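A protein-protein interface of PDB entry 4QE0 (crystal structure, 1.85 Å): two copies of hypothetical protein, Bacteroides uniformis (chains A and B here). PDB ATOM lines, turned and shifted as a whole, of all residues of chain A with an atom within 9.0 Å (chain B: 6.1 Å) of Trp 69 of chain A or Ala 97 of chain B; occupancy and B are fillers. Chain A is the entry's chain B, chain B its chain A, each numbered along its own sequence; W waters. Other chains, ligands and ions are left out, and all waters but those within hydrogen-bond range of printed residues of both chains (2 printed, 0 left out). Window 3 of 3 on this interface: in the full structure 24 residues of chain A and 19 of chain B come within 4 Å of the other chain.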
ATOM      1  N   TYR A  65      23.595  34.315  29.138  1.00  0.00           N
ATOM      2  CA  TYR A  65      23.808  32.919  29.438  1.00  0.00           C
ATOM      3  C   TYR A  65      24.891  32.436  28.500  1.00  0.00           C
ATOM      4  O   TYR A  65      24.711  32.432  27.298  1.00  0.00           O
ATOM      5  CB  TYR A  65      22.496  32.152  29.202  1.00  0.00           C
ATOM      6  CG  TYR A  65      22.573  30.713  29.485  1.00  0.00           C
ATOM      7  CD1 TYR A  65      22.513  30.252  30.787  1.00  0.00           C
ATOM      8  CD2 TYR A  65      22.730  29.792  28.459  1.00  0.00           C
ATOM      9  CE1 TYR A  65      22.600  28.903  31.063  1.00  0.00           C
ATOM     10  CE2 TYR A  65      22.809  28.454  28.730  1.00  0.00           C
ATOM     11  CZ  TYR A  65      22.745  28.023  30.041  1.00  0.00           C
ATOM     12  OH  TYR A  65      22.833  26.694  30.336  1.00  0.00           O
ATOM     13  N   ILE A  66      26.019  31.994  29.033  1.00  0.00           N
ATOM     14  CA  ILE A  66      27.166  31.620  28.177  1.00  0.00           C
ATOM     15  C   ILE A  66      27.084  30.181  27.669  1.00  0.00           C
ATOM     16  O   ILE A  66      27.572  29.820  26.557  1.00  0.00           O
ATOM     17  CB  ILE A  66      28.487  31.781  28.990  1.00  0.00           C
ATOM     18  CG1 ILE A  66      28.700  33.259  29.337  1.00  0.00           C
ATOM     19  CG2 ILE A  66      29.692  31.215  28.241  1.00  0.00           C
ATOM     20  CD1 ILE A  66      28.615  34.178  28.138  1.00  0.00           C
ATOM     21  N   GLY A  67      26.491  29.352  28.510  1.00  0.00           N
ATOM     22  CA  GLY A  67      26.415  27.929  28.259  1.00  0.00           C
ATOM     23  C   GLY A  67      27.544  27.215  28.980  1.00  0.00           C
ATOM     24  O   GLY A  67      28.691  27.676  29.016  1.00  0.00           O
ATOM     25  N   SER A  68      27.213  26.062  29.541  1.00  0.00           N
ATOM     26  CA  SER A  68      28.201  25.266  30.239  1.00  0.00           C
ATOM     27  C   SER A  68      27.685  23.825  30.341  1.00  0.00           C
ATOM     28  O   SER A  68      26.473  23.590  30.446  1.00  0.00           O
ATOM     29  CB  SER A  68      28.456  25.871  31.623  1.00  0.00           C
ATOM     30  OG  SER A  68      29.069  24.955  32.482  1.00  0.00           O
ATOM     31  N   TRP A  69      28.592  22.862  30.301  1.00  0.00           N
ATOM     32  CA  TRP A  69      28.202  21.472  30.557  1.00  0.00           C
ATOM     33  C   TRP A  69      27.611  21.335  31.951  1.00  0.00           C
ATOM     34  O   TRP A  69      26.844  20.402  32.194  1.00  0.00           O
ATOM     35  CB  TRP A  69      29.407  20.549  30.531  1.00  0.00           C
ATOM     36  CG  TRP A  69      30.044  20.396  29.199  1.00  0.00           C
ATOM     37  CD1 TRP A  69      31.331  20.659  28.889  1.00  0.00           C
ATOM     38  CD2 TRP A  69      29.421  19.939  28.004  1.00  0.00           C
ATOM     39  NE1 TRP A  69      31.558  20.402  27.570  1.00  0.00           N
ATOM     40  CE2 TRP A  69      30.403  19.944  26.998  1.00  0.00           C
ATOM     41  CE3 TRP A  69      28.125  19.505  27.684  1.00  0.00           C
ATOM     42  CZ2 TRP A  69      30.131  19.549  25.684  1.00  0.00           C
ATOM     43  CZ3 TRP A  69      27.850  19.112  26.380  1.00  0.00           C
ATOM     44  CH2 TRP A  69      28.846  19.139  25.393  1.00  0.00           C
ATOM     45  N   SER A  70      27.979  22.236  32.859  1.00  0.00           N
ATOM     46  CA  SER A  70      27.506  22.213  34.245  1.00  0.00           C
ATOM     47  C   SER A  70      26.130  22.853  34.444  1.00  0.00           C
ATOM     48  O   SER A  70      25.656  22.907  35.559  1.00  0.00           O
ATOM     49  CB  SER A  70      28.517  22.920  35.157  1.00  0.00           C
ATOM     50  OG  SER A  70      29.798  22.331  35.018  1.00  0.00           O
ATOM     51  N   SER A  71      25.528  23.376  33.386  1.00  0.00           N
ATOM     52  CA  SER A  71      24.240  24.037  33.466  1.00  0.00           C
ATOM     53  C   SER A  71      23.233  23.266  32.621  1.00  0.00           C
ATOM     54  O   SER A  71      23.313  23.246  31.393  1.00  0.00           O
ATOM     55  CB  SER A  71      24.384  25.485  33.001  1.00  0.00           C
ATOM     56  OG  SER A  71      23.102  26.066  32.902  1.00  0.00           O
ATOM     57  N   ASN A  72      22.272  22.625  33.275  1.00  0.00           N
ATOM     58  CA  ASN A  72      21.262  21.866  32.535  1.00  0.00           C
ATOM     59  C   ASN A  72      20.130  22.775  32.094  1.00  0.00           C
ATOM     60  O   ASN A  72      19.628  23.585  32.868  1.00  0.00           O
ATOM     61  CB  ASN A  72      20.647  20.798  33.413  1.00  0.00           C
ATOM     62  CG  ASN A  72      21.605  19.696  33.727  1.00  0.00           C
ATOM     63  OD1 ASN A  72      22.345  19.238  32.851  1.00  0.00           O
ATOM     64  ND2 ASN A  72      21.627  19.277  34.992  1.00  0.00           N
ATOM     65  N   VAL A  73      19.726  22.607  30.852  1.00  0.00           N
ATOM     66  CA  VAL A  73      18.585  23.339  30.311  1.00  0.00           C
ATOM     67  C   VAL A  73      17.425  22.422  29.898  1.00  0.00           C
ATOM     68  O   VAL A  73      16.285  22.835  29.921  1.00  0.00           O
ATOM     69  CB  VAL A  73      18.997  24.269  29.151  1.00  0.00           C
ATOM     70  CG1 VAL A  73      19.913  25.382  29.636  1.00  0.00           C
ATOM     71  CG2 VAL A  73      19.670  23.502  28.016  1.00  0.00           C
ATOM     72  N   GLU A 156      15.543  23.207  35.218  1.00  0.00           N
ATOM     73  CA  GLU A 156      16.641  23.927  35.875  1.00  0.00           C
ATOM     74  C   GLU A 156      16.881  25.281  35.222  1.00  0.00           C
ATOM     75  O   GLU A 156      15.932  26.058  35.135  1.00  0.00           O
ATOM     76  CB  GLU A 156      17.880  23.019  36.002  1.00  0.00           C
ATOM     77  CG  GLU A 156      17.530  21.784  36.840  1.00  0.00           C
ATOM     78  CD  GLU A 156      18.668  20.805  37.096  1.00  0.00           C
ATOM     79  OE1 GLU A 156      19.798  21.028  36.609  1.00  0.00           O
ATOM     80  OE2 GLU A 156      18.412  19.799  37.808  1.00  0.00           O
ATOM     81  N   GLU A 157      18.089  25.553  34.722  1.00  0.00           N
ATOM     82  CA  GLU A 157      18.382  26.874  34.164  1.00  0.00           C
ATOM     83  C   GLU A 157      17.587  27.169  32.902  1.00  0.00           C
ATOM     84  O   GLU A 157      17.306  28.331  32.600  1.00  0.00           O
ATOM     85  CB  GLU A 157      19.872  27.058  33.882  1.00  0.00           C
ATOM     86  CG  GLU A 157      20.774  26.635  35.053  1.00  0.00           C
ATOM     87  CD  GLU A 157      21.763  27.716  35.506  1.00  0.00           C
ATOM     88  OE1 GLU A 157      21.325  28.836  35.869  1.00  0.00           O
ATOM     89  OE2 GLU A 157      22.988  27.433  35.535  1.00  0.00           O
ATOM     90  N   ALA A 167      22.498  23.698  20.107  1.00  0.00           N
ATOM     91  CA  ALA A 167      23.309  23.808  18.887  1.00  0.00           C
ATOM     92  C   ALA A 167      24.259  22.631  18.877  1.00  0.00           C
ATOM     93  O   ALA A 167      24.810  22.285  19.922  1.00  0.00           O
ATOM     94  CB  ALA A 167      24.085  25.110  18.896  1.00  0.00           C
ATOM     95  N   TRP A 168      24.459  22.029  17.709  1.00  0.00           N
ATOM     96  CA  TRP A 168      25.414  20.942  17.566  1.00  0.00           C
ATOM     97  C   TRP A 168      26.011  20.899  16.178  1.00  0.00           C
ATOM     98  O   TRP A 168      25.489  21.508  15.231  1.00  0.00           O
ATOM     99  CB  TRP A 168      24.790  19.600  17.939  1.00  0.00           C
ATOM    100  CG  TRP A 168      23.865  18.977  16.952  1.00  0.00           C
ATOM    101  CD1 TRP A 168      24.137  17.924  16.116  1.00  0.00           C
ATOM    102  CD2 TRP A 168      22.512  19.357  16.684  1.00  0.00           C
ATOM    103  NE1 TRP A 168      23.041  17.610  15.364  1.00  0.00           N
ATOM    104  CE2 TRP A 168      22.019  18.459  15.700  1.00  0.00           C
ATOM    105  CE3 TRP A 168      21.663  20.337  17.201  1.00  0.00           C
ATOM    106  CZ2 TRP A 168      20.736  18.534  15.203  1.00  0.00           C
ATOM    107  CZ3 TRP A 168      20.369  20.424  16.698  1.00  0.00           C
ATOM    108  CH2 TRP A 168      19.922  19.527  15.705  1.00  0.00           C
ATOM    109  N   ASP B  89      36.818  24.902  22.604  1.00  0.00           N
ATOM    110  CA  ASP B  89      35.887  24.341  23.589  1.00  0.00           C
ATOM    111  C   ASP B  89      35.173  23.106  23.017  1.00  0.00           C
ATOM    112  O   ASP B  89      35.129  22.049  23.649  1.00  0.00           O
ATOM    113  CB  ASP B  89      34.877  25.399  23.976  1.00  0.00           C
ATOM    114  CG  ASP B  89      34.035  24.994  25.179  1.00  0.00           C
ATOM    115  OD1 ASP B  89      33.433  23.919  25.155  1.00  0.00           O
ATOM    116  OD2 ASP B  89      34.018  25.735  26.169  1.00  0.00           O
ATOM    117  N   PHE B  92      36.454  19.249  22.781  1.00  0.00           N
ATOM    118  CA  PHE B  92      36.415  18.388  23.956  1.00  0.00           C
ATOM    119  C   PHE B  92      34.993  17.922  24.252  1.00  0.00           C
ATOM    120  O   PHE B  92      34.060  18.729  24.238  1.00  0.00           O
ATOM    121  CB  PHE B  92      36.930  19.149  25.174  1.00  0.00           C
ATOM    122  CG  PHE B  92      38.390  19.495  25.106  1.00  0.00           C
ATOM    123  CD1 PHE B  92      38.815  20.639  24.448  1.00  0.00           C
ATOM    124  CD2 PHE B  92      39.336  18.713  25.743  1.00  0.00           C
ATOM    125  CE1 PHE B  92      40.162  20.965  24.380  1.00  0.00           C
ATOM    126  CE2 PHE B  92      40.688  19.039  25.677  1.00  0.00           C
ATOM    127  CZ  PHE B  92      41.094  20.157  24.988  1.00  0.00           C
ATOM    128  N   THR B  93      34.831  16.634  24.522  1.00  0.00           N
ATOM    129  CA  THR B  93      33.529  16.088  24.923  1.00  0.00           C
ATOM    130  C   THR B  93      33.207  16.531  26.347  1.00  0.00           C
ATOM    131  O   THR B  93      34.107  16.967  27.077  1.00  0.00           O
ATOM    132  CB  THR B  93      33.545  14.546  24.906  1.00  0.00           C
ATOM    133  OG1 THR B  93      34.527  14.068  25.837  1.00  0.00           O
ATOM    134  CG2 THR B  93      33.860  14.020  23.498  1.00  0.00           C
ATOM    135  N   MLY B  94      31.936  16.424  26.734  1.00  0.00           N
ATOM    136  CA  MLY B  94      31.506  16.678  28.113  1.00  0.00           C
ATOM    137  CB  MLY B  94      30.013  16.422  28.299  1.00  0.00           C
ATOM    138  CG  MLY B  94      29.552  16.650  29.741  1.00  0.00           C
ATOM    139  CD  MLY B  94      28.043  16.455  29.812  1.00  0.00           C
ATOM    140  CE  MLY B  94      27.455  16.875  31.169  1.00  0.00           C
ATOM    141  NZ  MLY B  94      28.029  16.068  32.284  1.00  0.00           N
ATOM    142  CH1 MLY B  94      27.387  16.350  33.604  1.00  0.00           C
ATOM    143  CH2 MLY B  94      27.931  14.595  32.054  1.00  0.00           C
ATOM    144  C   MLY B  94      32.302  15.809  29.051  1.00  0.00           C
ATOM    145  O   MLY B  94      32.771  16.288  30.076  1.00  0.00           O
ATOM    146  N   ALA B  95      32.513  14.542  28.692  1.00  0.00           N
ATOM    147  CA  ALA B  95      33.268  13.636  29.571  1.00  0.00           C
ATOM    148  C   ALA B  95      34.703  14.134  29.826  1.00  0.00           C
ATOM    149  O   ALA B  95      35.187  14.127  30.960  1.00  0.00           O
ATOM    150  CB  ALA B  95      33.279  12.233  28.995  1.00  0.00           C
ATOM    151  N   MET B  96      35.386  14.592  28.780  1.00  0.00           N
ATOM    152  CA  MET B  96      36.715  15.161  28.937  1.00  0.00           C
ATOM    153  C   MET B  96      36.676  16.424  29.757  1.00  0.00           C
ATOM    154  O   MET B  96      37.460  16.583  30.698  1.00  0.00           O
ATOM    155  CB  MET B  96      37.340  15.473  27.582  1.00  0.00           C
ATOM    156  CG  MET B  96      37.749  14.220  26.837  1.00  0.00           C
ATOM    157  SD  MET B  96      38.420  14.802  25.065  1.00  0.00           S
ATOM    158  CE  MET B  96      38.174  13.083  24.107  1.00  0.00           C
ATOM    159  N   ALA B  97      35.755  17.332  29.438  1.00  0.00           N
ATOM    160  CA  ALA B  97      35.714  18.621  30.116  1.00  0.00           C
ATOM    161  C   ALA B  97      35.451  18.434  31.613  1.00  0.00           C
ATOM    162  O   ALA B  97      36.068  19.100  32.454  1.00  0.00           O
ATOM    163  CB  ALA B  97      34.658  19.516  29.501  1.00  0.00           C
ATOM    164  N   ASP B  98      34.552  17.512  31.949  1.00  0.00           N
ATOM    165  CA  ASP B  98      34.245  17.198  33.355  1.00  0.00           C
ATOM    166  C   ASP B  98      35.455  16.645  34.112  1.00  0.00           C
ATOM    167  O   ASP B  98      35.637  16.943  35.285  1.00  0.00           O
ATOM    168  CB  ASP B  98      33.108  16.178  33.432  1.00  0.00           C
ATOM    169  CG  ASP B  98      31.738  16.776  33.115  1.00  0.00           C
ATOM    170  OD1 ASP B  98      31.607  18.007  33.041  1.00  0.00           O
ATOM    171  OD2 ASP B  98      30.770  15.991  32.949  1.00  0.00           O
ATOM    172  N   GLU B  99      36.295  15.869  33.431  1.00  0.00           N
ATOM    173  CA  GLU B  99      37.506  15.323  34.054  1.00  0.00           C
ATOM    174  C   GLU B  99      38.592  16.382  34.167  1.00  0.00           C
ATOM    175  O   GLU B  99      39.415  16.332  35.059  1.00  0.00           O
ATOM    176  CB  GLU B  99      38.051  14.141  33.259  1.00  0.00           C
ATOM    177  CG  GLU B  99      37.152  12.909  33.260  1.00  0.00           C
ATOM    178  CD  GLU B  99      37.639  11.821  32.304  1.00  0.00           C
ATOM    179  OE1 GLU B  99      37.502  11.977  31.056  1.00  0.00           O
ATOM    180  OE2 GLU B  99      38.151  10.801  32.807  1.00  0.00           O
ATOM    181  N   ILE B 100      38.601  17.336  33.244  1.00  0.00           N
ATOM    182  CA  ILE B 100      39.666  18.359  33.193  1.00  0.00           C
ATOM    183  C   ILE B 100      39.538  19.360  34.332  1.00  0.00           C
ATOM    184  O   ILE B 100      40.543  19.774  34.902  1.00  0.00           O
ATOM    185  CB  ILE B 100      39.669  19.076  31.835  1.00  0.00           C
ATOM    186  CG1 ILE B 100      40.320  18.170  30.812  1.00  0.00           C
ATOM    187  CG2 ILE B 100      40.419  20.409  31.909  1.00  0.00           C
ATOM    188  CD1 ILE B 100      40.036  18.553  29.375  1.00  0.00           C
ATOM    189  N   GLY B 101      38.307  19.728  34.684  1.00  0.00           N
ATOM    190  CA  GLY B 101      38.078  20.680  35.747  1.00  0.00           C
ATOM    191  C   GLY B 101      38.600  22.084  35.425  1.00  0.00           C
ATOM    192  O   GLY B 101      38.501  22.547  34.294  1.00  0.00           O
ATOM    193  N   PRO B 172      38.032  23.986  28.397  1.00  0.00           N
ATOM    194  CA  PRO B 172      36.731  23.640  27.789  1.00  0.00           C
ATOM    195  C   PRO B 172      35.655  23.598  28.857  1.00  0.00           C
ATOM    196  O   PRO B 172      35.875  23.029  29.920  1.00  0.00           O
ATOM    197  CB  PRO B 172      36.931  22.222  27.262  1.00  0.00           C
ATOM    198  CG  PRO B 172      38.105  21.675  27.994  1.00  0.00           C
ATOM    199  CD  PRO B 172      38.955  22.840  28.398  1.00  0.00           C
ATOM    200  N   GLN B 173      34.512  24.192  28.573  1.00  0.00           N
ATOM    201  CA  GLN B 173      33.424  24.261  29.554  1.00  0.00           C
ATOM    202  C   GLN B 173      32.044  23.980  28.947  1.00  0.00           C
ATOM    203  O   GLN B 173      31.094  23.931  29.672  1.00  0.00           O
ATOM    204  CB  GLN B 173      33.449  25.589  30.346  1.00  0.00           C
ATOM    205  CG  GLN B 173      33.872  26.832  29.584  1.00  0.00           C
ATOM    206  CD  GLN B 173      34.312  27.990  30.468  1.00  0.00           C
ATOM    207  OE1 GLN B 173      35.475  28.097  30.896  1.00  0.00           O
ATOM    208  NE2 GLN B 173      33.408  28.916  30.659  1.00  0.00           N
ATOM    209  N   GLY B 174      31.938  23.802  27.625  1.00  0.00           N
ATOM    210  CA  GLY B 174      30.635  23.517  27.003  1.00  0.00           C
ATOM    211  C   GLY B 174      29.850  24.790  26.674  1.00  0.00           C
ATOM    212  O   GLY B 174      28.633  24.847  26.789  1.00  0.00           O
ATOM    213  N   MLY B 175      30.563  25.811  26.239  1.00  0.00           N
ATOM    214  CA  MLY B 175      29.959  27.064  25.812  1.00  0.00           C
ATOM    215  CB  MLY B 175      31.014  28.096  25.485  1.00  0.00           C
ATOM    216  CG  MLY B 175      31.818  28.515  26.700  1.00  0.00           C
ATOM    217  CD  MLY B 175      32.810  29.602  26.302  1.00  0.00           C
ATOM    218  CE  MLY B 175      33.747  30.001  27.433  1.00  0.00           C
ATOM    219  NZ  MLY B 175      34.853  30.838  26.876  1.00  0.00           N
ATOM    220  CH1 MLY B 175      34.381  32.228  26.728  1.00  0.00           C
ATOM    221  CH2 MLY B 175      36.023  30.808  27.760  1.00  0.00           C
ATOM    222  C   MLY B 175      29.122  26.885  24.565  1.00  0.00           C
ATOM    223  O   MLY B 175      29.406  26.035  23.717  1.00  0.00           O
HETATM  224  O   HOH W   1      31.229  22.870  32.610  1.00  0.00           O
HETATM  225  O   HOH W   2      33.689  21.007  25.813  1.00  0.00           O
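Hydrophobic or aromatic side chains of chain B within 4 Å of the printed part of chain A: Ala 97. Hydrophobic or aromatic side chains of chain A within 4 Å of the printed part of chain B: Ile 66 and Trp 69. Among the printed residues, no Asp or Glu carboxylate lies within 4 Å of a Lys or Arg side-chain nitrogen of the other chain.
Water W2 lies within hydrogen-bond range of the backbone carbonyl oxygen (O) of Phe 92 of chain B, the backbone carbonyl oxygen (O) of Asp 89 of chain B and the indole nitrogen (NE1) of Trp 69 of chain A. Water W1 lies within hydrogen-bond range of the side-chain hydroxyl of Ser 70 of chain A (2.9 Å), the side-chain hydroxyl of Ser 68 of chain A (3.0 Å) and the backbone carbonyl oxygen of Gln 173 of chain B (3.1 Å).
Among the printed residues, merely in contact across the chains: Ile 66 of chain A with MLY 175 of chain B, Gly 67 of chain A with Gly 174 of chain B, Gly 67 of chain A with MLY 175 of chain B, Ser 68 of chain A with Gln 173 of chain B, Trp 69 of chain A with MLY 94 of chain B and Trp 69 of chain A with Ala 97 of chain B.
O of Gln 173 of chain B is in hydrogen-bond range of N of Trp 69 of chain A, at 2.8 Å. The backbone carbonyl oxygen of Gly 174 of chain B lies within hydrogen-bond range of the backbone NH of Ser 68 of chain A (3.3 Å). The indole nitrogen (NE1) of Trp 69 of chain A lies close to the backbone NH (N) of Gly 174 of chain B (3.4 Å).
Printed residues of chain B within 4 Å of Trp 69 of chain A: MLY 94, Ala 97, Gln 173 and Gly 174. Of chain A, only Trp 69 comes within 4 Å of Ala 97 of chain B. No residue of chain A comes within 4 Å of Gly 101 of chain B. Of chain A, only Gly 67, Ser 68 and Trp 69 come within 4 Å of Gly 174 of chain B. Printed residues of chain A within 4 Å of MLY 94 of chain B: Trp 69. Of the printed residues of chain B, Gly 67 of chain A touches Gly 174 (3.4 Å) and MLY 175 (3.5 Å). Printed residues of chain A within 4 Å of Gln 173 of chain B: Ser 68 (3.2 Å) and Trp 69 (2.8 Å). Of the printed residues of chain A, MLY 175 of chain B touches Ile 66 (3.7 Å) and Gly 67 (3.5 Å). Of the printed residues of chain B, Ile 66 of chain A touches MLY 175. The nearest printed residue of chain A that does not touch Ala 97 of chain B is Ser 70 of chain A (7.5 Å). The nearest printed residue of chain A that does not touch MLY 94 of chain B is Ser 70 of chain A (5.6 Å).
The backbone NH (N) of Gln 173 of chain B is in hydrogen-bond range of the side-chain carboxylate (OD2) of Asp 89 of chain B (2.9 Å). The backbone NH (N) of Gly 174 of chain B is in hydrogen-bond range of the side-chain carboxylate (OD1) of Asp 89 of chain B (2.9 Å). OD2 of Asp 89 of chain B sits at hydrogen-bond distance from N of MLY 175 of chain B (3.5 Å). NZ of MLY 94 of chain B lies close to the side-chain carboxylate of Asp 98 of chain B (2.8 Å). The side-chain hydroxyl (OG) of Ser 68 of chain A lies within hydrogen-bond range of the backbone NH (N) of Ser 70 of chain A.
No position is printed for both chains. Of the 9 pairs that touch across the chains among the printed residues, none has its exchanged pair printed and touching as well.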
